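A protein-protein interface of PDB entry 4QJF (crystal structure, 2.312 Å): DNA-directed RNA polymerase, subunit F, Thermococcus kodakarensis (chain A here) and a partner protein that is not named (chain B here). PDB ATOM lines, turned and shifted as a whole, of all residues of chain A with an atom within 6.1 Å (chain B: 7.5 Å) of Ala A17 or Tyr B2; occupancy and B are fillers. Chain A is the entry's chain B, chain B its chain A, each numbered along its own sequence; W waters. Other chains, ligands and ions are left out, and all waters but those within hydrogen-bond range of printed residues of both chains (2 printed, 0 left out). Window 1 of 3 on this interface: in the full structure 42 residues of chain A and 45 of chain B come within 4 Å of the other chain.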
ATOM      1  N   HIS A  10     -22.496  -2.198  -2.490  1.00  0.00           N
ATOM      2  CA  HIS A  10     -23.861  -2.043  -2.975  1.00  0.00           C
ATOM      3  C   HIS A  10     -24.886  -2.314  -1.888  1.00  0.00           C
ATOM      4  O   HIS A  10     -24.665  -3.147  -1.018  1.00  0.00           O
ATOM      5  CB  HIS A  10     -24.111  -2.965  -4.169  1.00  0.00           C
ATOM      6  CG  HIS A  10     -23.323  -2.595  -5.384  1.00  0.00           C
ATOM      7  ND1 HIS A  10     -23.835  -1.805  -6.395  1.00  0.00           N
ATOM      8  CD2 HIS A  10     -22.049  -2.888  -5.746  1.00  0.00           C
ATOM      9  CE1 HIS A  10     -22.919  -1.643  -7.328  1.00  0.00           C
ATOM     10  NE2 HIS A  10     -21.826  -2.290  -6.958  1.00  0.00           N
ATOM     11  N   TYR A  11     -26.002  -1.595  -1.942  1.00  0.00           N
ATOM     12  CA  TYR A  11     -27.123  -1.857  -1.059  1.00  0.00           C
ATOM     13  C   TYR A  11     -27.983  -2.937  -1.685  1.00  0.00           C
ATOM     14  O   TYR A  11     -28.358  -2.854  -2.849  1.00  0.00           O
ATOM     15  CB  TYR A  11     -27.927  -0.586  -0.793  1.00  0.00           C
ATOM     16  CG  TYR A  11     -27.163   0.417   0.032  1.00  0.00           C
ATOM     17  CD1 TYR A  11     -26.354   1.389  -0.576  1.00  0.00           C
ATOM     18  CD2 TYR A  11     -27.219   0.381   1.426  1.00  0.00           C
ATOM     19  CE1 TYR A  11     -25.636   2.326   0.202  1.00  0.00           C
ATOM     20  CE2 TYR A  11     -26.498   1.294   2.203  1.00  0.00           C
ATOM     21  CZ  TYR A  11     -25.712   2.261   1.594  1.00  0.00           C
ATOM     22  OH  TYR A  11     -25.019   3.149   2.387  1.00  0.00           O
ATOM     23  N   ILE A  12     -28.280  -3.955  -0.898  1.00  0.00           N
ATOM     24  CA  ILE A  12     -28.843  -5.195  -1.411  1.00  0.00           C
ATOM     25  C   ILE A  12     -30.199  -5.429  -0.741  1.00  0.00           C
ATOM     26  O   ILE A  12     -30.422  -4.973   0.375  1.00  0.00           O
ATOM     27  CB  ILE A  12     -27.836  -6.354  -1.159  1.00  0.00           C
ATOM     28  CG1 ILE A  12     -26.629  -6.200  -2.087  1.00  0.00           C
ATOM     29  CG2 ILE A  12     -28.434  -7.702  -1.352  1.00  0.00           C
ATOM     30  CD1 ILE A  12     -26.965  -6.260  -3.537  1.00  0.00           C
ATOM     31  N   THR A  13     -31.119  -6.086  -1.437  1.00  0.00           N
ATOM     32  CA  THR A  13     -32.406  -6.438  -0.842  1.00  0.00           C
ATOM     33  C   THR A  13     -32.312  -7.662   0.060  1.00  0.00           C
ATOM     34  O   THR A  13     -31.350  -8.437  -0.007  1.00  0.00           O
ATOM     35  CB  THR A  13     -33.455  -6.747  -1.893  1.00  0.00           C
ATOM     36  OG1 THR A  13     -33.046  -7.903  -2.644  1.00  0.00           O
ATOM     37  CG2 THR A  13     -33.672  -5.551  -2.810  1.00  0.00           C
ATOM     38  N   ILE A  14     -33.330  -7.833   0.894  1.00  0.00           N
ATOM     39  CA  ILE A  14     -33.470  -9.027   1.713  1.00  0.00           C
ATOM     40  C   ILE A  14     -33.542 -10.276   0.808  1.00  0.00           C
ATOM     41  O   ILE A  14     -32.910 -11.301   1.093  1.00  0.00           O
ATOM     42  CB  ILE A  14     -34.730  -8.919   2.621  1.00  0.00           C
ATOM     43  CG1 ILE A  14     -34.527  -7.823   3.682  1.00  0.00           C
ATOM     44  CG2 ILE A  14     -35.088 -10.264   3.254  1.00  0.00           C
ATOM     45  CD1 ILE A  14     -35.711  -7.631   4.636  1.00  0.00           C
ATOM     46  N   ALA A  15     -34.295 -10.172  -0.291  1.00  0.00           N
ATOM     47  CA  ALA A  15     -34.417 -11.272  -1.253  1.00  0.00           C
ATOM     48  C   ALA A  15     -33.049 -11.696  -1.811  1.00  0.00           C
ATOM     49  O   ALA A  15     -32.726 -12.880  -1.813  1.00  0.00           O
ATOM     50  CB  ALA A  15     -35.375 -10.888  -2.396  1.00  0.00           C
ATOM     51  N   GLU A  16     -32.242 -10.740  -2.267  1.00  0.00           N
ATOM     52  CA  GLU A  16     -30.905 -11.087  -2.752  1.00  0.00           C
ATOM     53  C   GLU A  16     -30.080 -11.718  -1.633  1.00  0.00           C
ATOM     54  O   GLU A  16     -29.316 -12.654  -1.868  1.00  0.00           O
ATOM     55  CB  GLU A  16     -30.168  -9.863  -3.306  1.00  0.00           C
ATOM     56  CG  GLU A  16     -30.704  -9.302  -4.619  1.00  0.00           C
ATOM     57  CD  GLU A  16     -30.297  -7.841  -4.832  1.00  0.00           C
ATOM     58  OE1 GLU A  16     -31.067  -6.938  -4.459  1.00  0.00           O
ATOM     59  OE2 GLU A  16     -29.204  -7.592  -5.370  1.00  0.00           O
ATOM     60  N   ALA A  17     -30.247 -11.212  -0.412  1.00  0.00           N
ATOM     61  CA  ALA A  17     -29.452 -11.688   0.711  1.00  0.00           C
ATOM     62  C   ALA A  17     -29.849 -13.119   1.107  1.00  0.00           C
ATOM     63  O   ALA A  17     -28.994 -13.939   1.463  1.00  0.00           O
ATOM     64  CB  ALA A  17     -29.581 -10.724   1.900  1.00  0.00           C
ATOM     65  N   LYS A  18     -31.141 -13.418   1.016  1.00  0.00           N
ATOM     66  CA  LYS A  18     -31.635 -14.784   1.191  1.00  0.00           C
ATOM     67  C   LYS A  18     -30.905 -15.781   0.286  1.00  0.00           C
ATOM     68  O   LYS A  18     -30.494 -16.847   0.736  1.00  0.00           O
ATOM     69  CB  LYS A  18     -33.144 -14.855   0.920  1.00  0.00           C
ATOM     70  CG  LYS A  18     -33.760 -16.248   1.070  1.00  0.00           C
ATOM     71  CD  LYS A  18     -35.297 -16.169   0.995  1.00  0.00           C
ATOM     72  CE  LYS A  18     -35.851 -16.701  -0.330  1.00  0.00           C
ATOM     73  NZ  LYS A  18     -36.549 -18.014  -0.166  1.00  0.00           N
ATOM     74  N   GLU A  19     -30.743 -15.428  -0.984  1.00  0.00           N
ATOM     75  CA  GLU A  19     -30.031 -16.306  -1.899  1.00  0.00           C
ATOM     76  C   GLU A  19     -28.586 -16.518  -1.436  1.00  0.00           C
ATOM     77  O   GLU A  19     -28.122 -17.659  -1.352  1.00  0.00           O
ATOM     78  CB  GLU A  19     -30.063 -15.755  -3.327  1.00  0.00           C
ATOM     79  CG  GLU A  19     -29.308 -16.621  -4.337  1.00  0.00           C
ATOM     80  CD  GLU A  19     -29.498 -16.182  -5.774  1.00  0.00           C
ATOM     81  OE1 GLU A  19     -28.989 -16.878  -6.672  1.00  0.00           O
ATOM     82  OE2 GLU A  19     -30.149 -15.144  -6.015  1.00  0.00           O
ATOM     83  N   LEU A  20     -27.897 -15.427  -1.109  1.00  0.00           N
ATOM     84  CA  LEU A  20     -26.501 -15.515  -0.688  1.00  0.00           C
ATOM     85  C   LEU A  20     -26.360 -16.263   0.633  1.00  0.00           C
ATOM     86  O   LEU A  20     -25.424 -17.048   0.810  1.00  0.00           O
ATOM     87  CB  LEU A  20     -25.878 -14.126  -0.568  1.00  0.00           C
ATOM     88  CG  LEU A  20     -25.949 -13.251  -1.817  1.00  0.00           C
ATOM     89  CD1 LEU A  20     -25.459 -11.836  -1.518  1.00  0.00           C
ATOM     90  CD2 LEU A  20     -25.141 -13.886  -2.956  1.00  0.00           C
ATOM     91  N   LEU A  21     -27.285 -16.044   1.562  1.00  0.00           N
ATOM     92  CA  LEU A  21     -27.191 -16.750   2.840  1.00  0.00           C
ATOM     93  C   LEU A  21     -27.362 -18.255   2.664  1.00  0.00           C
ATOM     94  O   LEU A  21     -26.649 -19.032   3.298  1.00  0.00           O
ATOM     95  CB  LEU A  21     -28.205 -16.212   3.835  1.00  0.00           C
ATOM     96  CG  LEU A  21     -27.819 -14.814   4.308  1.00  0.00           C
ATOM     97  CD1 LEU A  21     -28.989 -14.148   5.012  1.00  0.00           C
ATOM     98  CD2 LEU A  21     -26.570 -14.871   5.201  1.00  0.00           C
ATOM     99  N   GLU A  22     -28.288 -18.650   1.791  1.00  0.00           N
ATOM    100  CA  GLU A  22     -28.518 -20.065   1.507  1.00  0.00           C
ATOM    101  C   GLU A  22     -27.280 -20.687   0.860  1.00  0.00           C
ATOM    102  O   GLU A  22     -26.949 -21.835   1.148  1.00  0.00           O
ATOM    103  CB  GLU A  22     -29.752 -20.258   0.611  1.00  0.00           C
ATOM    104  CG  GLU A  22     -31.074 -20.091   1.339  1.00  0.00           C
ATOM    105  CD  GLU A  22     -32.244 -19.913   0.398  1.00  0.00           C
ATOM    106  OE1 GLU A  22     -32.019 -19.780  -0.824  1.00  0.00           O
ATOM    107  OE2 GLU A  22     -33.393 -19.897   0.874  1.00  0.00           O
ATOM    108  N   SER A  44     -30.181 -14.452  10.873  1.00  0.00           N
ATOM    109  CA  SER A  44     -30.354 -13.615   9.706  1.00  0.00           C
ATOM    110  C   SER A  44     -30.968 -14.414   8.558  1.00  0.00           C
ATOM    111  O   SER A  44     -31.914 -13.943   7.905  1.00  0.00           O
ATOM    112  CB  SER A  44     -29.014 -13.016   9.272  1.00  0.00           C
ATOM    113  OG  SER A  44     -29.222 -11.789   8.615  1.00  0.00           O
ATOM    114  N   LEU A  45     -30.415 -15.605   8.312  1.00  0.00           N
ATOM    115  CA  LEU A  45     -30.957 -16.513   7.303  1.00  0.00           C
ATOM    116  C   LEU A  45     -32.471 -16.757   7.504  1.00  0.00           C
ATOM    117  O   LEU A  45     -33.232 -16.630   6.549  1.00  0.00           O
ATOM    118  CB  LEU A  45     -30.201 -17.846   7.305  1.00  0.00           C
ATOM    119  CG  LEU A  45     -30.732 -18.955   6.367  1.00  0.00           C
ATOM    120  CD1 LEU A  45     -31.100 -18.475   4.952  1.00  0.00           C
ATOM    121  CD2 LEU A  45     -29.730 -20.086   6.280  1.00  0.00           C
ATOM    122  N   HIS A  47     -34.784 -14.987   9.318  1.00  0.00           N
ATOM    123  CA  HIS A  47     -35.450 -13.726   9.056  1.00  0.00           C
ATOM    124  C   HIS A  47     -35.609 -13.496   7.558  1.00  0.00           C
ATOM    125  O   HIS A  47     -36.702 -13.206   7.080  1.00  0.00           O
ATOM    126  CB  HIS A  47     -34.686 -12.555   9.684  1.00  0.00           C
ATOM    127  CG  HIS A  47     -35.457 -11.271   9.673  1.00  0.00           C
ATOM    128  ND1 HIS A  47     -35.329 -10.335   8.670  1.00  0.00           N
ATOM    129  CD2 HIS A  47     -36.402 -10.794  10.519  1.00  0.00           C
ATOM    130  CE1 HIS A  47     -36.143  -9.321   8.913  1.00  0.00           C
ATOM    131  NE2 HIS A  47     -36.800  -9.573  10.031  1.00  0.00           N
ATOM    132  N   ALA A  48     -34.513 -13.643   6.825  1.00  0.00           N
ATOM    133  CA  ALA A  48     -34.526 -13.383   5.392  1.00  0.00           C
ATOM    134  C   ALA A  48     -35.458 -14.363   4.677  1.00  0.00           C
ATOM    135  O   ALA A  48     -36.164 -13.971   3.757  1.00  0.00           O
ATOM    136  CB  ALA A  48     -33.117 -13.454   4.820  1.00  0.00           C
ATOM    137  N   ASP A  83     -37.684  -4.166  -0.229  1.00  0.00           N
ATOM    138  CA  ASP A  83     -37.880  -4.927   1.003  1.00  0.00           C
ATOM    139  C   ASP A  83     -39.257  -4.677   1.599  1.00  0.00           C
ATOM    140  O   ASP A  83     -39.943  -5.623   2.009  1.00  0.00           O
ATOM    141  CB  ASP A  83     -36.806  -4.589   2.041  1.00  0.00           C
ATOM    142  CG  ASP A  83     -35.416  -5.112   1.655  1.00  0.00           C
ATOM    143  OD1 ASP A  83     -35.313  -5.952   0.737  1.00  0.00           O
ATOM    144  OD2 ASP A  83     -34.429  -4.695   2.292  1.00  0.00           O
ATOM    145  N   MET B   1     -30.892  -3.838   6.511  1.00  0.00           N
ATOM    146  CA  MET B   1     -29.942  -3.102   5.692  1.00  0.00           C
ATOM    147  C   MET B   1     -28.755  -3.976   5.278  1.00  0.00           C
ATOM    148  O   MET B   1     -27.649  -3.817   5.793  1.00  0.00           O
ATOM    149  CB  MET B   1     -29.451  -1.870   6.449  1.00  0.00           C
ATOM    150  CG  MET B   1     -28.599  -0.903   5.633  1.00  0.00           C
ATOM    151  SD  MET B   1     -29.406   0.675   5.367  1.00  0.00           S
ATOM    152  CE  MET B   1     -27.956   1.660   5.083  1.00  0.00           C
ATOM    153  N   TYR B   2     -28.984  -4.889   4.339  1.00  0.00           N
ATOM    154  CA  TYR B   2     -27.921  -5.756   3.845  1.00  0.00           C
ATOM    155  C   TYR B   2     -27.024  -5.031   2.849  1.00  0.00           C
ATOM    156  O   TYR B   2     -27.509  -4.243   2.033  1.00  0.00           O
ATOM    157  CB  TYR B   2     -28.513  -6.993   3.168  1.00  0.00           C
ATOM    158  CG  TYR B   2     -29.081  -8.052   4.081  1.00  0.00           C
ATOM    159  CD1 TYR B   2     -30.449  -8.186   4.257  1.00  0.00           C
ATOM    160  CD2 TYR B   2     -28.249  -8.948   4.730  1.00  0.00           C
ATOM    161  CE1 TYR B   2     -30.972  -9.178   5.061  1.00  0.00           C
ATOM    162  CE2 TYR B   2     -28.750  -9.932   5.533  1.00  0.00           C
ATOM    163  CZ  TYR B   2     -30.114 -10.045   5.700  1.00  0.00           C
ATOM    164  OH  TYR B   2     -30.606 -11.032   6.500  1.00  0.00           O
ATOM    165  N   LYS B   3     -25.724  -5.305   2.887  1.00  0.00           N
ATOM    166  CA  LYS B   3     -24.826  -4.750   1.861  1.00  0.00           C
ATOM    167  C   LYS B   3     -23.839  -5.778   1.321  1.00  0.00           C
ATOM    168  O   LYS B   3     -23.438  -6.714   2.026  1.00  0.00           O
ATOM    169  CB  LYS B   3     -24.038  -3.537   2.399  1.00  0.00           C
ATOM    170  CG  LYS B   3     -24.873  -2.309   2.779  1.00  0.00           C
ATOM    171  CD  LYS B   3     -24.069  -1.339   3.631  1.00  0.00           C
ATOM    172  CE  LYS B   3     -22.900  -0.728   2.847  1.00  0.00           C
ATOM    173  NZ  LYS B   3     -22.133   0.324   3.601  1.00  0.00           N
ATOM    174  N   LEU B   4     -23.438  -5.573   0.066  1.00  0.00           N
ATOM    175  CA  LEU B   4     -22.416  -6.387  -0.591  1.00  0.00           C
ATOM    176  C   LEU B   4     -21.135  -5.581  -0.815  1.00  0.00           C
ATOM    177  O   LEU B   4     -21.115  -4.615  -1.590  1.00  0.00           O
ATOM    178  CB  LEU B   4     -22.945  -6.909  -1.924  1.00  0.00           C
ATOM    179  CG  LEU B   4     -22.594  -8.296  -2.459  1.00  0.00           C
ATOM    180  CD1 LEU B   4     -23.164  -8.493  -3.881  1.00  0.00           C
ATOM    181  CD2 LEU B   4     -21.107  -8.524  -2.442  1.00  0.00           C
ATOM    182  N   VAL B  44     -22.450  -6.049  10.935  1.00  0.00           N
ATOM    183  CA  VAL B  44     -22.347  -7.502  11.073  1.00  0.00           C
ATOM    184  C   VAL B  44     -21.731  -8.143   9.838  1.00  0.00           C
ATOM    185  O   VAL B  44     -22.261  -7.980   8.750  1.00  0.00           O
ATOM    186  CB  VAL B  44     -23.743  -8.172  11.312  1.00  0.00           C
ATOM    187  CG1 VAL B  44     -23.607  -9.690  11.337  1.00  0.00           C
ATOM    188  CG2 VAL B  44     -24.375  -7.684  12.608  1.00  0.00           C
ATOM    189  N   LEU B  46     -21.522 -11.203   7.824  1.00  0.00           N
ATOM    190  CA  LEU B  46     -22.326 -12.422   7.762  1.00  0.00           C
ATOM    191  C   LEU B  46     -21.659 -13.550   6.964  1.00  0.00           C
ATOM    192  O   LEU B  46     -21.721 -14.707   7.378  1.00  0.00           O
ATOM    193  CB  LEU B  46     -23.695 -12.126   7.166  1.00  0.00           C
ATOM    194  CG  LEU B  46     -24.651 -11.321   8.044  1.00  0.00           C
ATOM    195  CD1 LEU B  46     -25.786 -10.699   7.220  1.00  0.00           C
ATOM    196  CD2 LEU B  46     -25.203 -12.189   9.133  1.00  0.00           C
ATOM    197  N   LEU B  49     -18.362 -14.498   0.684  1.00  0.00           N
ATOM    198  CA  LEU B  49     -19.144 -15.172  -0.357  1.00  0.00           C
ATOM    199  C   LEU B  49     -18.252 -15.930  -1.324  1.00  0.00           C
ATOM    200  O   LEU B  49     -18.492 -17.101  -1.600  1.00  0.00           O
ATOM    201  CB  LEU B  49     -20.019 -14.173  -1.122  1.00  0.00           C
ATOM    202  CG  LEU B  49     -20.956 -13.367  -0.210  1.00  0.00           C
ATOM    203  CD1 LEU B  49     -21.503 -12.143  -0.936  1.00  0.00           C
ATOM    204  CD2 LEU B  49     -22.092 -14.242   0.341  1.00  0.00           C
ATOM    205  N   LEU B  75     -20.806 -10.369   2.402  1.00  0.00           N
ATOM    206  CA  LEU B  75     -22.133  -9.947   2.830  1.00  0.00           C
ATOM    207  C   LEU B  75     -22.084  -9.409   4.258  1.00  0.00           C
ATOM    208  O   LEU B  75     -21.572 -10.059   5.164  1.00  0.00           O
ATOM    209  CB  LEU B  75     -23.146 -11.086   2.726  1.00  0.00           C
ATOM    210  CG  LEU B  75     -24.570 -10.732   3.182  1.00  0.00           C
ATOM    211  CD1 LEU B  75     -25.303  -9.777   2.198  1.00  0.00           C
ATOM    212  CD2 LEU B  75     -25.362 -11.995   3.403  1.00  0.00           C
ATOM    213  N   VAL B  76     -22.608  -8.206   4.441  1.00  0.00           N
ATOM    214  CA  VAL B  76     -22.710  -7.600   5.758  1.00  0.00           C
ATOM    215  C   VAL B  76     -24.129  -7.083   5.952  1.00  0.00           C
ATOM    216  O   VAL B  76     -24.920  -7.080   5.019  1.00  0.00           O
ATOM    217  CB  VAL B  76     -21.701  -6.441   5.949  1.00  0.00           C
ATOM    218  CG1 VAL B  76     -20.253  -6.932   5.783  1.00  0.00           C
ATOM    219  CG2 VAL B  76     -22.009  -5.308   4.969  1.00  0.00           C
ATOM    220  N   TRP B  77     -24.439  -6.650   7.169  1.00  0.00           N
ATOM    221  CA  TRP B  77     -25.742  -6.099   7.517  1.00  0.00           C
ATOM    222  C   TRP B  77     -25.511  -5.029   8.556  1.00  0.00           C
ATOM    223  O   TRP B  77     -24.810  -5.266   9.544  1.00  0.00           O
ATOM    224  CB  TRP B  77     -26.685  -7.185   8.071  1.00  0.00           C
ATOM    225  CG  TRP B  77     -28.096  -6.708   8.478  1.00  0.00           C
ATOM    226  CD1 TRP B  77     -29.229  -6.730   7.701  1.00  0.00           C
ATOM    227  CD2 TRP B  77     -28.504  -6.174   9.752  1.00  0.00           C
ATOM    228  NE1 TRP B  77     -30.307  -6.259   8.413  1.00  0.00           N
ATOM    229  CE2 TRP B  77     -29.891  -5.904   9.673  1.00  0.00           C
ATOM    230  CE3 TRP B  77     -27.834  -5.899  10.953  1.00  0.00           C
ATOM    231  CZ2 TRP B  77     -30.613  -5.362  10.734  1.00  0.00           C
ATOM    232  CZ3 TRP B  77     -28.556  -5.378  12.012  1.00  0.00           C
ATOM    233  CH2 TRP B  77     -29.933  -5.117  11.897  1.00  0.00           C
ATOM    234  N   GLU B  78     -26.109  -3.861   8.367  1.00  0.00           N
ATOM    235  CA  GLU B  78     -25.929  -2.802   9.344  1.00  0.00           C
ATOM    236  C   GLU B  78     -27.248  -2.239   9.837  1.00  0.00           C
ATOM    237  O   GLU B  78     -28.184  -2.073   9.069  1.00  0.00           O
ATOM    238  CB  GLU B  78     -25.066  -1.684   8.764  1.00  0.00           C
ATOM    239  CG  GLU B  78     -25.832  -0.562   8.098  1.00  0.00           C
ATOM    240  CD  GLU B  78     -24.914   0.521   7.572  1.00  0.00           C
ATOM    241  OE1 GLU B  78     -25.404   1.381   6.798  1.00  0.00           O
ATOM    242  OE2 GLU B  78     -23.707   0.502   7.931  1.00  0.00           O
ATOM    243  N   GLU B  83     -33.490   4.189   9.927  1.00  0.00           N
ATOM    244  CA  GLU B  83     -33.884   3.222   8.915  1.00  0.00           C
ATOM    245  C   GLU B  83     -35.218   2.507   9.240  1.00  0.00           C
ATOM    246  O   GLU B  83     -35.480   2.090  10.364  1.00  0.00           O
ATOM    247  CB  GLU B  83     -32.775   2.196   8.714  1.00  0.00           C
ATOM    248  CG  GLU B  83     -33.161   1.025   7.843  1.00  0.00           C
ATOM    249  CD  GLU B  83     -32.176  -0.138   7.967  1.00  0.00           C
ATOM    250  OE1 GLU B  83     -31.251  -0.087   8.816  1.00  0.00           O
ATOM    251  OE2 GLU B  83     -32.335  -1.104   7.206  1.00  0.00           O
ATOM    252  N   ILE B 101     -34.922  -8.247  13.477  1.00  0.00           N
ATOM    253  CA  ILE B 101     -34.961  -7.445  12.247  1.00  0.00           C
ATOM    254  C   ILE B 101     -33.890  -7.567  11.131  1.00  0.00           C
ATOM    255  O   ILE B 101     -33.915  -6.725  10.252  1.00  0.00           O
ATOM    256  CB  ILE B 101     -34.955  -5.916  12.589  1.00  0.00           C
ATOM    257  CG1 ILE B 101     -33.588  -5.454  13.086  1.00  0.00           C
ATOM    258  CG2 ILE B 101     -36.070  -5.526  13.584  1.00  0.00           C
ATOM    259  CD1 ILE B 101     -33.429  -3.931  13.053  1.00  0.00           C
ATOM    260  N   GLY B 102     -32.985  -8.555  11.080  1.00  0.00           N
ATOM    261  CA  GLY B 102     -32.990  -9.776  11.858  1.00  0.00           C
ATOM    262  C   GLY B 102     -31.711 -10.538  12.222  1.00  0.00           C
ATOM    263  O   GLY B 102     -31.834 -11.525  12.921  1.00  0.00           O
ATOM    264  N   PRO B 103     -30.503 -10.131  11.769  1.00  0.00           N
ATOM    265  CA  PRO B 103     -29.392 -10.796  12.479  1.00  0.00           C
ATOM    266  C   PRO B 103     -29.200 -10.229  13.896  1.00  0.00           C
ATOM    267  O   PRO B 103     -28.513 -10.836  14.718  1.00  0.00           O
ATOM    268  CB  PRO B 103     -28.165 -10.519  11.595  1.00  0.00           C
ATOM    269  CG  PRO B 103     -28.518  -9.353  10.784  1.00  0.00           C
ATOM    270  CD  PRO B 103     -30.025  -9.346  10.615  1.00  0.00           C
HETATM  271  O   HOH W   1     -31.399  -5.343   2.633  1.00  0.00           O
HETATM  272  O   HOH W   2     -33.346 -10.665   6.787  1.00  0.00           O
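The backbone NH (N) of Ile A12 sits at hydrogen-bond distance from the backbone carbonyl oxygen (O) of Tyr B2 (3.0 Å). The backbone NH of His A10 lies within hydrogen-bond range of the backbone carbonyl oxygen of Leu B4, 2.9 Å away. The side-chain hydroxyl of Tyr B2 sits at hydrogen-bond distance from the side-chain hydroxyl of Ser A44.
The backbone NH (N) of Met B1 sits close to the side-chain carboxylate (OE2) of Glu B83, 3.2 Å away. O of Val B76 is in hydrogen-bond range of N of Lys B3, at 2.9 Å. The backbone NH (N) of Glu B78 is in hydrogen-bond range of the backbone carbonyl oxygen (O) of Met B1 (3.0 Å). N of Leu B46 sits at hydrogen-bond distance from O of Leu B75.
CE2 of Tyr A11 touches CE of Met B1, 3.2 Å away. Tyr A11 touches Tyr B2. Ile A12 touches Leu B4 (CG1 to CB, 3.8 Å). Tyr B2 touches Ala A17 (CG to CB, 3.5 Å). CB of Leu A20 touches CD2 of Leu B49, 3.9 Å away. Leu A21 touches Tyr B2 (CD1 to OH, 3.8 Å). OG of Ser A44 touches CD1 of Leu B46 (3.9 Å). N of Ser A44 touches O of Gly B102, 3.9 Å away. NE2 of His A47 touches CA of Ile B101 (3.6 Å). Gly B102 touches His A47 (CA to CG, 3.6 Å).
Of the printed residues of chain B, Ala A17 touches Tyr B2 (3.5 Å). Tyr B2 touches just these residues of chain A: Tyr A11, Ile A12, Ala A17, Leu A21, Ser A44 and Ala A48. Printed residues of chain A within 4 Å of Met B1: Tyr A11 (3.2 Å). Of the printed residues of chain B, Leu A21 touches Tyr B2 and Leu B75. Ile A14 touches none of the printed residues of chain B.
Of the 15 printed residues of chain B, 10 touch a printed residue of chain A. Printed residues of chain B that touch a printed residue of chain A: Met B1, Tyr B2, Lys B3, Leu B4, Leu B46, Leu B49, Leu B75, Ile B101, Gly B102 and Pro B103. Printed residues of chain A that touch a printed residue of chain B: His A10, Tyr A11, Ile A12, Ala A17, Leu A20, Leu A21, Ser A44, His A47 and Ala A48. Hydrophobic or aromatic side chains of chain A that line the printed part of chain B: Tyr A11, Ile A12, Ala A17, Leu A20, Leu A21, His A47 and Ala A48. Along chain A the printed residues that touch a printed residue of chain B span positions 10 to 48. Among the printed residues, no Asp or Glu carboxylate lies within 4 Å of a Lys or Arg side-chain nitrogen of the other chain.
Water W1 lies within hydrogen-bond range of the backbone carbonyl oxygen of Ile A12, the backbone NH of Tyr B2 and the side-chain carboxylate of Asp A83. Water W2 lies within hydrogen-bond range of a ring nitrogen (ND1) of His A47 (2.8 Å), the side-chain hydroxyl of Tyr B2 (2.8 Å) and the backbone NH of Ala A48 (3.2 Å).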
